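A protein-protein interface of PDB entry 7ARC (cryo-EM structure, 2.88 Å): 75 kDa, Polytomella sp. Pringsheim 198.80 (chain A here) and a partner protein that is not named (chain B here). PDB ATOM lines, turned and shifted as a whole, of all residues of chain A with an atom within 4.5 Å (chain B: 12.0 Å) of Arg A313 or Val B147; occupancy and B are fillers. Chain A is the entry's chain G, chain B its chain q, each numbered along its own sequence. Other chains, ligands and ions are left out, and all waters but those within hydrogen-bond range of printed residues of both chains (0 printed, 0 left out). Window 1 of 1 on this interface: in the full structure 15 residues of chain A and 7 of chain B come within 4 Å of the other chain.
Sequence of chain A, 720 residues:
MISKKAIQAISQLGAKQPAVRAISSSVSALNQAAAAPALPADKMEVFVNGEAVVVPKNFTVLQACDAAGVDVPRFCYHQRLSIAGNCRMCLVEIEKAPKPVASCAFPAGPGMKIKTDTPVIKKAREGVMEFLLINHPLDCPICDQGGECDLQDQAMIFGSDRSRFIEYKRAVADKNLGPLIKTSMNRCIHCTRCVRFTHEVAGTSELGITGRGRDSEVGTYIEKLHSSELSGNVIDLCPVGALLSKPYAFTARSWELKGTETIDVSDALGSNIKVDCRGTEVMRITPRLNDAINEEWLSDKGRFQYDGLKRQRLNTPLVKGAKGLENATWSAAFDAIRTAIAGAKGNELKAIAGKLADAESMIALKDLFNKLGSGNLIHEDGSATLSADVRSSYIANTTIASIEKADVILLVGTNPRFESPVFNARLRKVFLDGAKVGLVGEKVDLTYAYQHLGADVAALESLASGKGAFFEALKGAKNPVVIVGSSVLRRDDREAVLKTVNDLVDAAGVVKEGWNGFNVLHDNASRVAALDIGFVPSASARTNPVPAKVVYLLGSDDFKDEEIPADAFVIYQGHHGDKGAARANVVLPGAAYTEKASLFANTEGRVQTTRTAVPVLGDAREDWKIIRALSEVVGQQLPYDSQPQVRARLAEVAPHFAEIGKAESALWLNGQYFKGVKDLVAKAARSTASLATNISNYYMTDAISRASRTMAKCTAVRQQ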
ATOM      1  N   LEU A 309     -21.656   1.656  11.216  1.00  0.00           N
ATOM      2  CA  LEU A 309     -21.318   1.912  12.606  1.00  0.00           C
ATOM      3  C   LEU A 309     -21.298   0.640  13.435  1.00  0.00           C
ATOM      4  O   LEU A 309     -21.001   0.701  14.631  1.00  0.00           O
ATOM      5  CB  LEU A 309     -22.306   2.903  13.225  1.00  0.00           C
ATOM      6  CG  LEU A 309     -21.930   4.380  13.174  1.00  0.00           C
ATOM      7  CD1 LEU A 309     -23.161   5.229  13.410  1.00  0.00           C
ATOM      8  CD2 LEU A 309     -20.847   4.696  14.183  1.00  0.00           C
ATOM      9  N   LYS A 310     -21.608  -0.505  12.831  1.00  0.00           N
ATOM     10  CA  LYS A 310     -21.611  -1.777  13.530  1.00  0.00           C
ATOM     11  C   LYS A 310     -20.469  -2.677  13.087  1.00  0.00           C
ATOM     12  O   LYS A 310     -20.353  -3.798  13.587  1.00  0.00           O
ATOM     13  CB  LYS A 310     -22.935  -2.511  13.289  1.00  0.00           C
ATOM     14  CG  LYS A 310     -24.114  -2.048  14.125  1.00  0.00           C
ATOM     15  CD  LYS A 310     -24.619  -0.703  13.639  1.00  0.00           C
ATOM     16  CE  LYS A 310     -25.851  -0.251  14.384  1.00  0.00           C
ATOM     17  NZ  LYS A 310     -26.244   1.118  13.960  1.00  0.00           N
ATOM     18  N   ARG A 311     -19.626  -2.214  12.171  1.00  0.00           N
ATOM     19  CA  ARG A 311     -18.661  -3.061  11.492  1.00  0.00           C
ATOM     20  C   ARG A 311     -17.274  -2.442  11.579  1.00  0.00           C
ATOM     21  O   ARG A 311     -17.128  -1.220  11.501  1.00  0.00           O
ATOM     22  CB  ARG A 311     -19.066  -3.260  10.028  1.00  0.00           C
ATOM     23  CG  ARG A 311     -18.164  -4.189   9.248  1.00  0.00           C
ATOM     24  CD  ARG A 311     -18.660  -4.372   7.830  1.00  0.00           C
ATOM     25  NE  ARG A 311     -17.812  -5.293   7.085  1.00  0.00           N
ATOM     26  CZ  ARG A 311     -16.751  -4.928   6.382  1.00  0.00           C
ATOM     27  NH1 ARG A 311     -16.374  -3.662   6.307  1.00  0.00           N
ATOM     28  NH2 ARG A 311     -16.048  -5.856   5.739  1.00  0.00           N
ATOM     29  N   GLN A 312     -16.261  -3.296  11.734  1.00  0.00           N
ATOM     30  CA  GLN A 312     -14.855  -2.882  11.772  1.00  0.00           C
ATOM     31  C   GLN A 312     -14.601  -1.851  12.869  1.00  0.00           C
ATOM     32  O   GLN A 312     -13.823  -0.912  12.696  1.00  0.00           O
ATOM     33  CB  GLN A 312     -14.410  -2.341  10.411  1.00  0.00           C
ATOM     34  CG  GLN A 312     -14.446  -3.356   9.280  1.00  0.00           C
ATOM     35  CD  GLN A 312     -13.388  -4.428   9.411  1.00  0.00           C
ATOM     36  OE1 GLN A 312     -12.293  -4.306   8.864  1.00  0.00           O
ATOM     37  NE2 GLN A 312     -13.711  -5.495  10.130  1.00  0.00           N
ATOM     38  N   ARG A 313     -15.250  -2.035  14.013  1.00  0.00           N
ATOM     39  CA  ARG A 313     -15.141  -1.096  15.119  1.00  0.00           C
ATOM     40  C   ARG A 313     -13.929  -1.391  15.990  1.00  0.00           C
ATOM     41  O   ARG A 313     -13.553  -2.550  16.191  1.00  0.00           O
ATOM     42  CB  ARG A 313     -16.416  -1.110  15.957  1.00  0.00           C
ATOM     43  CG  ARG A 313     -17.629  -0.611  15.197  1.00  0.00           C
ATOM     44  CD  ARG A 313     -17.501   0.848  14.820  1.00  0.00           C
ATOM     45  NE  ARG A 313     -17.051   1.665  15.938  1.00  0.00           N
ATOM     46  CZ  ARG A 313     -17.859   2.238  16.818  1.00  0.00           C
ATOM     47  NH1 ARG A 313     -19.173   2.119  16.730  1.00  0.00           N
ATOM     48  NH2 ARG A 313     -17.336   2.952  17.809  1.00  0.00           N
ATOM     49  N   LEU A 314     -13.313  -0.330  16.502  1.00  0.00           N
ATOM     50  CA  LEU A 314     -12.226  -0.440  17.465  1.00  0.00           C
ATOM     51  C   LEU A 314     -12.792  -0.359  18.875  1.00  0.00           C
ATOM     52  O   LEU A 314     -13.486   0.604  19.216  1.00  0.00           O
ATOM     53  CB  LEU A 314     -11.199   0.669  17.252  1.00  0.00           C
ATOM     54  CG  LEU A 314     -10.460   0.723  15.921  1.00  0.00           C
ATOM     55  CD1 LEU A 314      -9.622   1.982  15.849  1.00  0.00           C
ATOM     56  CD2 LEU A 314      -9.599  -0.497  15.769  1.00  0.00           C
ATOM     57  N   ASN A 315     -12.497  -1.367  19.691  1.00  0.00           N
ATOM     58  CA  ASN A 315     -13.033  -1.456  21.040  1.00  0.00           C
ATOM     59  C   ASN A 315     -11.978  -1.351  22.131  1.00  0.00           C
ATOM     60  O   ASN A 315     -12.300  -0.902  23.230  1.00  0.00           O
ATOM     61  CB  ASN A 315     -13.813  -2.768  21.222  1.00  0.00           C
ATOM     62  CG  ASN A 315     -12.944  -3.994  21.048  1.00  0.00           C
ATOM     63  OD1 ASN A 315     -11.967  -3.974  20.304  1.00  0.00           O
ATOM     64  ND2 ASN A 315     -13.296  -5.072  21.735  1.00  0.00           N
ATOM     65  N   HIS A 575     -12.251   5.354  15.670  1.00  0.00           N
ATOM     66  CA  HIS A 575     -13.328   4.436  15.993  1.00  0.00           C
ATOM     67  C   HIS A 575     -13.590   3.338  14.968  1.00  0.00           C
ATOM     68  O   HIS A 575     -14.307   2.387  15.292  1.00  0.00           O
ATOM     69  CB  HIS A 575     -14.609   5.239  16.277  1.00  0.00           C
ATOM     70  CG  HIS A 575     -15.084   6.063  15.125  1.00  0.00           C
ATOM     71  ND1 HIS A 575     -15.912   5.574  14.140  1.00  0.00           N
ATOM     72  CD2 HIS A 575     -14.838   7.355  14.800  1.00  0.00           C
ATOM     73  CE1 HIS A 575     -16.159   6.529  13.261  1.00  0.00           C
ATOM     74  NE2 HIS A 575     -15.518   7.619  13.638  1.00  0.00           N
ATOM     75  N   HIS A 576     -13.034   3.420  13.762  1.00  0.00           N
ATOM     76  CA  HIS A 576     -13.042   2.306  12.822  1.00  0.00           C
ATOM     77  C   HIS A 576     -11.627   1.886  12.460  1.00  0.00           C
ATOM     78  O   HIS A 576     -10.701   2.700  12.448  1.00  0.00           O
ATOM     79  CB  HIS A 576     -13.795   2.627  11.523  1.00  0.00           C
ATOM     80  CG  HIS A 576     -15.283   2.609  11.659  1.00  0.00           C
ATOM     81  ND1 HIS A 576     -16.003   3.681  12.132  1.00  0.00           N
ATOM     82  CD2 HIS A 576     -16.187   1.646  11.374  1.00  0.00           C
ATOM     83  CE1 HIS A 576     -17.288   3.378  12.141  1.00  0.00           C
ATOM     84  NE2 HIS A 576     -17.427   2.148  11.683  1.00  0.00           N
ATOM     85  N   GLY A 590     -11.771   5.369  20.140  1.00  0.00           N
ATOM     86  CA  GLY A 590     -12.499   6.579  20.436  1.00  0.00           C
ATOM     87  C   GLY A 590     -13.964   6.425  20.077  1.00  0.00           C
ATOM     88  O   GLY A 590     -14.357   5.515  19.352  1.00  0.00           O
ATOM     89  N   GLU A 595     -21.863   8.676  19.565  1.00  0.00           N
ATOM     90  CA  GLU A 595     -21.552   8.273  20.926  1.00  0.00           C
ATOM     91  C   GLU A 595     -20.926   9.379  21.763  1.00  0.00           C
ATOM     92  O   GLU A 595     -20.551   9.123  22.912  1.00  0.00           O
ATOM     93  CB  GLU A 595     -20.612   7.065  20.890  1.00  0.00           C
ATOM     94  CG  GLU A 595     -21.253   5.817  20.331  1.00  0.00           C
ATOM     95  CD  GLU A 595     -20.307   4.639  20.283  1.00  0.00           C
ATOM     96  OE1 GLU A 595     -19.107   4.829  20.570  1.00  0.00           O
ATOM     97  OE2 GLU A 595     -20.762   3.522  19.961  1.00  0.00           O
ATOM     98  N   LEU A 617     -18.615   1.995  23.088  1.00  0.00           N
ATOM     99  CA  LEU A 617     -18.453   0.555  22.954  1.00  0.00           C
ATOM    100  C   LEU A 617     -17.129   0.099  23.546  1.00  0.00           C
ATOM    101  O   LEU A 617     -16.082   0.692  23.269  1.00  0.00           O
ATOM    102  CB  LEU A 617     -18.511   0.153  21.481  1.00  0.00           C
ATOM    103  CG  LEU A 617     -18.416  -1.343  21.205  1.00  0.00           C
ATOM    104  CD1 LEU A 617     -19.591  -2.091  21.815  1.00  0.00           C
ATOM    105  CD2 LEU A 617     -18.310  -1.589  19.722  1.00  0.00           C
ATOM    106  N   ARG B 142     -23.318 -17.976  23.404  1.00  0.00           N
ATOM    107  CA  ARG B 142     -23.541 -16.725  22.693  1.00  0.00           C
ATOM    108  C   ARG B 142     -23.200 -15.552  23.601  1.00  0.00           C
ATOM    109  O   ARG B 142     -23.763 -15.429  24.694  1.00  0.00           O
ATOM    110  CB  ARG B 142     -24.990 -16.613  22.225  1.00  0.00           C
ATOM    111  CG  ARG B 142     -25.380 -17.620  21.174  1.00  0.00           C
ATOM    112  CD  ARG B 142     -26.418 -17.053  20.236  1.00  0.00           C
ATOM    113  NE  ARG B 142     -26.821 -18.033  19.235  1.00  0.00           N
ATOM    114  CZ  ARG B 142     -27.867 -17.894  18.433  1.00  0.00           C
ATOM    115  NH1 ARG B 142     -28.599 -16.793  18.438  1.00  0.00           N
ATOM    116  NH2 ARG B 142     -28.177 -18.880  17.597  1.00  0.00           N
ATOM    117  N   ASN B 143     -22.278 -14.701  23.156  1.00  0.00           N
ATOM    118  CA  ASN B 143     -22.149 -13.350  23.691  1.00  0.00           C
ATOM    119  C   ASN B 143     -22.934 -12.414  22.772  1.00  0.00           C
ATOM    120  O   ASN B 143     -22.577 -12.208  21.611  1.00  0.00           O
ATOM    121  CB  ASN B 143     -20.683 -12.947  23.904  1.00  0.00           C
ATOM    122  CG  ASN B 143     -19.839 -12.898  22.620  1.00  0.00           C
ATOM    123  OD1 ASN B 143     -18.630 -12.704  22.632  1.00  0.00           O
ATOM    124  ND2 ASN B 143     -20.511 -13.093  21.492  1.00  0.00           N
ATOM    125  N   TRP B 144     -24.027 -11.863  23.290  1.00  0.00           N
ATOM    126  CA  TRP B 144     -24.980 -11.145  22.448  1.00  0.00           C
ATOM    127  C   TRP B 144     -24.486  -9.726  22.164  1.00  0.00           C
ATOM    128  O   TRP B 144     -25.100  -8.725  22.526  1.00  0.00           O
ATOM    129  CB  TRP B 144     -26.355 -11.141  23.098  1.00  0.00           C
ATOM    130  CG  TRP B 144     -26.744 -12.454  23.712  1.00  0.00           C
ATOM    131  CD1 TRP B 144     -26.279 -12.986  24.877  1.00  0.00           C
ATOM    132  CD2 TRP B 144     -27.685 -13.396  23.191  1.00  0.00           C
ATOM    133  NE1 TRP B 144     -26.869 -14.200  25.113  1.00  0.00           N
ATOM    134  CE2 TRP B 144     -27.738 -14.475  24.091  1.00  0.00           C
ATOM    135  CE3 TRP B 144     -28.486 -13.435  22.048  1.00  0.00           C
ATOM    136  CZ2 TRP B 144     -28.560 -15.577  23.886  1.00  0.00           C
ATOM    137  CZ3 TRP B 144     -29.302 -14.527  21.849  1.00  0.00           C
ATOM    138  CH2 TRP B 144     -29.333 -15.583  22.761  1.00  0.00           C
ATOM    139  N   LYS B 145     -23.350  -9.668  21.477  1.00  0.00           N
ATOM    140  CA  LYS B 145     -22.756  -8.411  21.053  1.00  0.00           C
ATOM    141  C   LYS B 145     -23.272  -8.063  19.665  1.00  0.00           C
ATOM    142  O   LYS B 145     -23.281  -8.909  18.768  1.00  0.00           O
ATOM    143  CB  LYS B 145     -21.231  -8.505  21.043  1.00  0.00           C
ATOM    144  CG  LYS B 145     -20.564  -8.820  22.386  1.00  0.00           C
ATOM    145  CD  LYS B 145     -20.634  -7.661  23.380  1.00  0.00           C
ATOM    146  CE  LYS B 145     -21.829  -7.752  24.317  1.00  0.00           C
ATOM    147  NZ  LYS B 145     -21.812  -6.672  25.342  1.00  0.00           N
ATOM    148  N   LYS B 146     -23.714  -6.821  19.499  1.00  0.00           N
ATOM    149  CA  LYS B 146     -24.339  -6.372  18.266  1.00  0.00           C
ATOM    150  C   LYS B 146     -23.390  -5.578  17.385  1.00  0.00           C
ATOM    151  O   LYS B 146     -23.843  -4.888  16.468  1.00  0.00           O
ATOM    152  CB  LYS B 146     -25.587  -5.546  18.577  1.00  0.00           C
ATOM    153  CG  LYS B 146     -26.746  -6.373  19.098  1.00  0.00           C
ATOM    154  CD  LYS B 146     -27.976  -5.523  19.338  1.00  0.00           C
ATOM    155  CE  LYS B 146     -28.101  -5.135  20.796  1.00  0.00           C
ATOM    156  NZ  LYS B 146     -29.207  -4.165  21.010  1.00  0.00           N
ATOM    157  N   VAL B 147     -22.088  -5.639  17.647  1.00  0.00           N
ATOM    158  CA  VAL B 147     -21.098  -4.936  16.844  1.00  0.00           C
ATOM    159  C   VAL B 147     -19.979  -5.899  16.479  1.00  0.00           C
ATOM    160  O   VAL B 147     -19.493  -6.645  17.335  1.00  0.00           O
ATOM    161  CB  VAL B 147     -20.529  -3.713  17.586  1.00  0.00           C
ATOM    162  CG1 VAL B 147     -19.441  -3.082  16.766  1.00  0.00           C
ATOM    163  CG2 VAL B 147     -21.625  -2.702  17.865  1.00  0.00           C
ATOM    164  N   GLU B 148     -19.582  -5.885  15.210  1.00  0.00           N
ATOM    165  CA  GLU B 148     -18.427  -6.644  14.754  1.00  0.00           C
ATOM    166  C   GLU B 148     -17.154  -5.851  15.024  1.00  0.00           C
ATOM    167  O   GLU B 148     -17.099  -4.642  14.789  1.00  0.00           O
ATOM    168  CB  GLU B 148     -18.557  -6.965  13.265  1.00  0.00           C
ATOM    169  CG  GLU B 148     -17.439  -7.824  12.711  1.00  0.00           C
ATOM    170  CD  GLU B 148     -17.637  -8.157  11.245  1.00  0.00           C
ATOM    171  OE1 GLU B 148     -18.641  -7.695  10.662  1.00  0.00           O
ATOM    172  OE2 GLU B 148     -16.792  -8.879  10.675  1.00  0.00           O
ATOM    173  N   ILE B 149     -16.130  -6.536  15.522  1.00  0.00           N
ATOM    174  CA  ILE B 149     -14.900  -5.893  15.970  1.00  0.00           C
ATOM    175  C   ILE B 149     -13.804  -6.110  14.937  1.00  0.00           C
ATOM    176  O   ILE B 149     -13.661  -7.206  14.381  1.00  0.00           O
ATOM    177  CB  ILE B 149     -14.479  -6.428  17.351  1.00  0.00           C
ATOM    178  CG1 ILE B 149     -15.522  -6.051  18.402  1.00  0.00           C
ATOM    179  CG2 ILE B 149     -13.118  -5.891  17.750  1.00  0.00           C
ATOM    180  CD1 ILE B 149     -15.842  -4.580  18.443  1.00  0.00           C
ATOM    181  N   TRP B 150     -13.034  -5.056  14.675  1.00  0.00           N
ATOM    182  CA  TRP B 150     -11.942  -5.117  13.712  1.00  0.00           C
ATOM    183  C   TRP B 150     -10.880  -6.113  14.156  1.00  0.00           C
ATOM    184  O   TRP B 150     -10.452  -6.109  15.313  1.00  0.00           O
ATOM    185  CB  TRP B 150     -11.328  -3.728  13.560  1.00  0.00           C
ATOM    186  CG  TRP B 150     -10.234  -3.616  12.549  1.00  0.00           C
ATOM    187  CD1 TRP B 150     -10.341  -3.791  11.204  1.00  0.00           C
ATOM    188  CD2 TRP B 150      -8.866  -3.276  12.802  1.00  0.00           C
ATOM    189  NE1 TRP B 150      -9.125  -3.590  10.602  1.00  0.00           N
ATOM    190  CE2 TRP B 150      -8.203  -3.273  11.562  1.00  0.00           C
ATOM    191  CE3 TRP B 150      -8.138  -2.984  13.956  1.00  0.00           C
ATOM    192  CZ2 TRP B 150      -6.848  -2.985  11.445  1.00  0.00           C
ATOM    193  CZ3 TRP B 150      -6.796  -2.696  13.837  1.00  0.00           C
ATOM    194  CH2 TRP B 150      -6.163  -2.700  12.592  1.00  0.00           C
ATOM    195  N   GLN B 151     -10.446  -6.965  13.227  1.00  0.00           N
ATOM    196  CA  GLN B 151      -9.383  -7.917  13.500  1.00  0.00           C
ATOM    197  C   GLN B 151      -8.075  -7.385  12.939  1.00  0.00           C
ATOM    198  O   GLN B 151      -7.997  -7.129  11.728  1.00  0.00           O
ATOM    199  CB  GLN B 151      -9.704  -9.276  12.891  1.00  0.00           C
ATOM    200  CG  GLN B 151     -10.861 -10.021  13.555  1.00  0.00           C
ATOM    201  CD  GLN B 151     -10.815  -9.976  15.074  1.00  0.00           C
ATOM    202  OE1 GLN B 151     -11.828  -9.732  15.727  1.00  0.00           O
ATOM    203  NE2 GLN B 151      -9.644 -10.245  15.643  1.00  0.00           N
ATOM    204  N   PRO B 152      -7.048  -7.189  13.762  1.00  0.00           N
ATOM    205  CA  PRO B 152      -5.826  -6.569  13.264  1.00  0.00           C
ATOM    206  C   PRO B 152      -5.162  -7.445  12.225  1.00  0.00           C
ATOM    207  O   PRO B 152      -5.271  -8.685  12.269  1.00  0.00           O
ATOM    208  CB  PRO B 152      -4.962  -6.434  14.526  1.00  0.00           C
ATOM    209  CG  PRO B 152      -5.940  -6.459  15.648  1.00  0.00           C
ATOM    210  CD  PRO B 152      -6.981  -7.432  15.210  1.00  0.00           C
ATOM    211  N   PRO B 153      -4.468  -6.847  11.258  1.00  0.00           N
ATOM    212  CA  PRO B 153      -3.747  -7.648  10.264  1.00  0.00           C
ATOM    213  C   PRO B 153      -2.628  -8.450  10.910  1.00  0.00           C
ATOM    214  O   PRO B 153      -2.039  -8.045  11.914  1.00  0.00           O
ATOM    215  CB  PRO B 153      -3.197  -6.599   9.291  1.00  0.00           C
ATOM    216  CG  PRO B 153      -4.033  -5.378   9.530  1.00  0.00           C
ATOM    217  CD  PRO B 153      -4.343  -5.406  10.991  1.00  0.00           C
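Of the 12 printed residues of chain A, 7 touch a printed residue of chain B. Printed residues of chain B that touch a printed residue of chain A: Lys B146, Val B147, Glu B148, Ile B149 and Trp B150. Hydrophobic or aromatic side chains of chain B within 4 Å of the printed part of chain A: Val B147, Ile B149 and Trp B150. Along chain B the printed residues that touch a printed residue of chain A span positions 146 to 150. Among the printed residues, 13 pairs touch across the chains. Among the printed residues, no Asp or Glu carboxylate lies within 4 Å of a Lys or Arg side-chain nitrogen of the other chain.
The backbone carbonyl oxygen (O) of Ile B149 sits close to the side-chain amide oxygen (OE1) of Gln B151 (3.4 Å). The backbone carbonyl oxygen of Leu A309 sits at hydrogen-bond distance from the guanidinium group of Arg A313 (3.1 Å). O of Arg A311 sits close to NE2 of His A576 (3.4 Å). The backbone carbonyl oxygen of His A575 sits at hydrogen-bond distance from the guanidinium group of Arg A313 (2.9 Å). The guanidinium group of Arg A313 is in salt-bridge range of the side-chain carboxylate of Glu A595, at 3.8 Å. The backbone carbonyl oxygen of His A575 lies within hydrogen-bond range of the backbone NH of Leu A314 (3.1 Å).
The backbone NH of Glu B148 lies within hydrogen-bond range of the backbone carbonyl oxygen of Lys A310 (2.8 Å). The backbone carbonyl oxygen of Glu B148 sits at hydrogen-bond distance from the backbone NH of Gln A312, at 3.4 Å. N of Arg A313 is in hydrogen-bond range of O of Glu B148. The backbone NH (N) of Trp B150 lies within hydrogen-bond range of the backbone carbonyl oxygen (O) of Arg A313 (3.0 Å).
O of Lys B146 touches CG of Lys A310, 3.7 Å away. O of Lys A310 touches CG1 of Val B147, at 3.4 Å. Glu B148 touches Arg A311. Gln A312 touches Trp B150 (OE1 to CD1, 3.1 Å). Val B147 touches Arg A313. Arg A313 touches Ile B149. CD2 of Leu A314 touches CE3 of Trp B150, at 3.4 Å. OD1 of Asn A315 touches CG2 of Ile B149, 3.4 Å away. CD2 of Leu A617 touches CG1 of Val B147, at 3.5 Å.
Arg A313 touches four residues of chain B. Val B147 touches three residues of chain A. No residue of chain B comes within 4 Å of Leu A309. Lys A310 touches just these residues of chain B: Lys B146, Val B147 and Glu B148. Of chain B, only Glu B148 (3.4 Å) and Trp B150 (3.1 Å) come within 4 Å of Gln A312. No residue of chain B comes within 4 Å of Gly A590. Leu A617 touches just one residue of chain B: Val B147 (3.5 Å). Of the printed residues of chain A, Ile B149 touches Arg A313 (3.6 Å) and Asn A315 (3.4 Å). Of the printed residues of chain A, Lys B146 touches Lys A310 (3.7 Å). Trp B144 touches none of the printed residues of chain A. The nearest residue of chain B that does not touch Arg A313 is Gln B151 (6.2 Å). The nearest printed residue of chain A that does not touch Val B147 is Leu A309 (4.6 Å).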
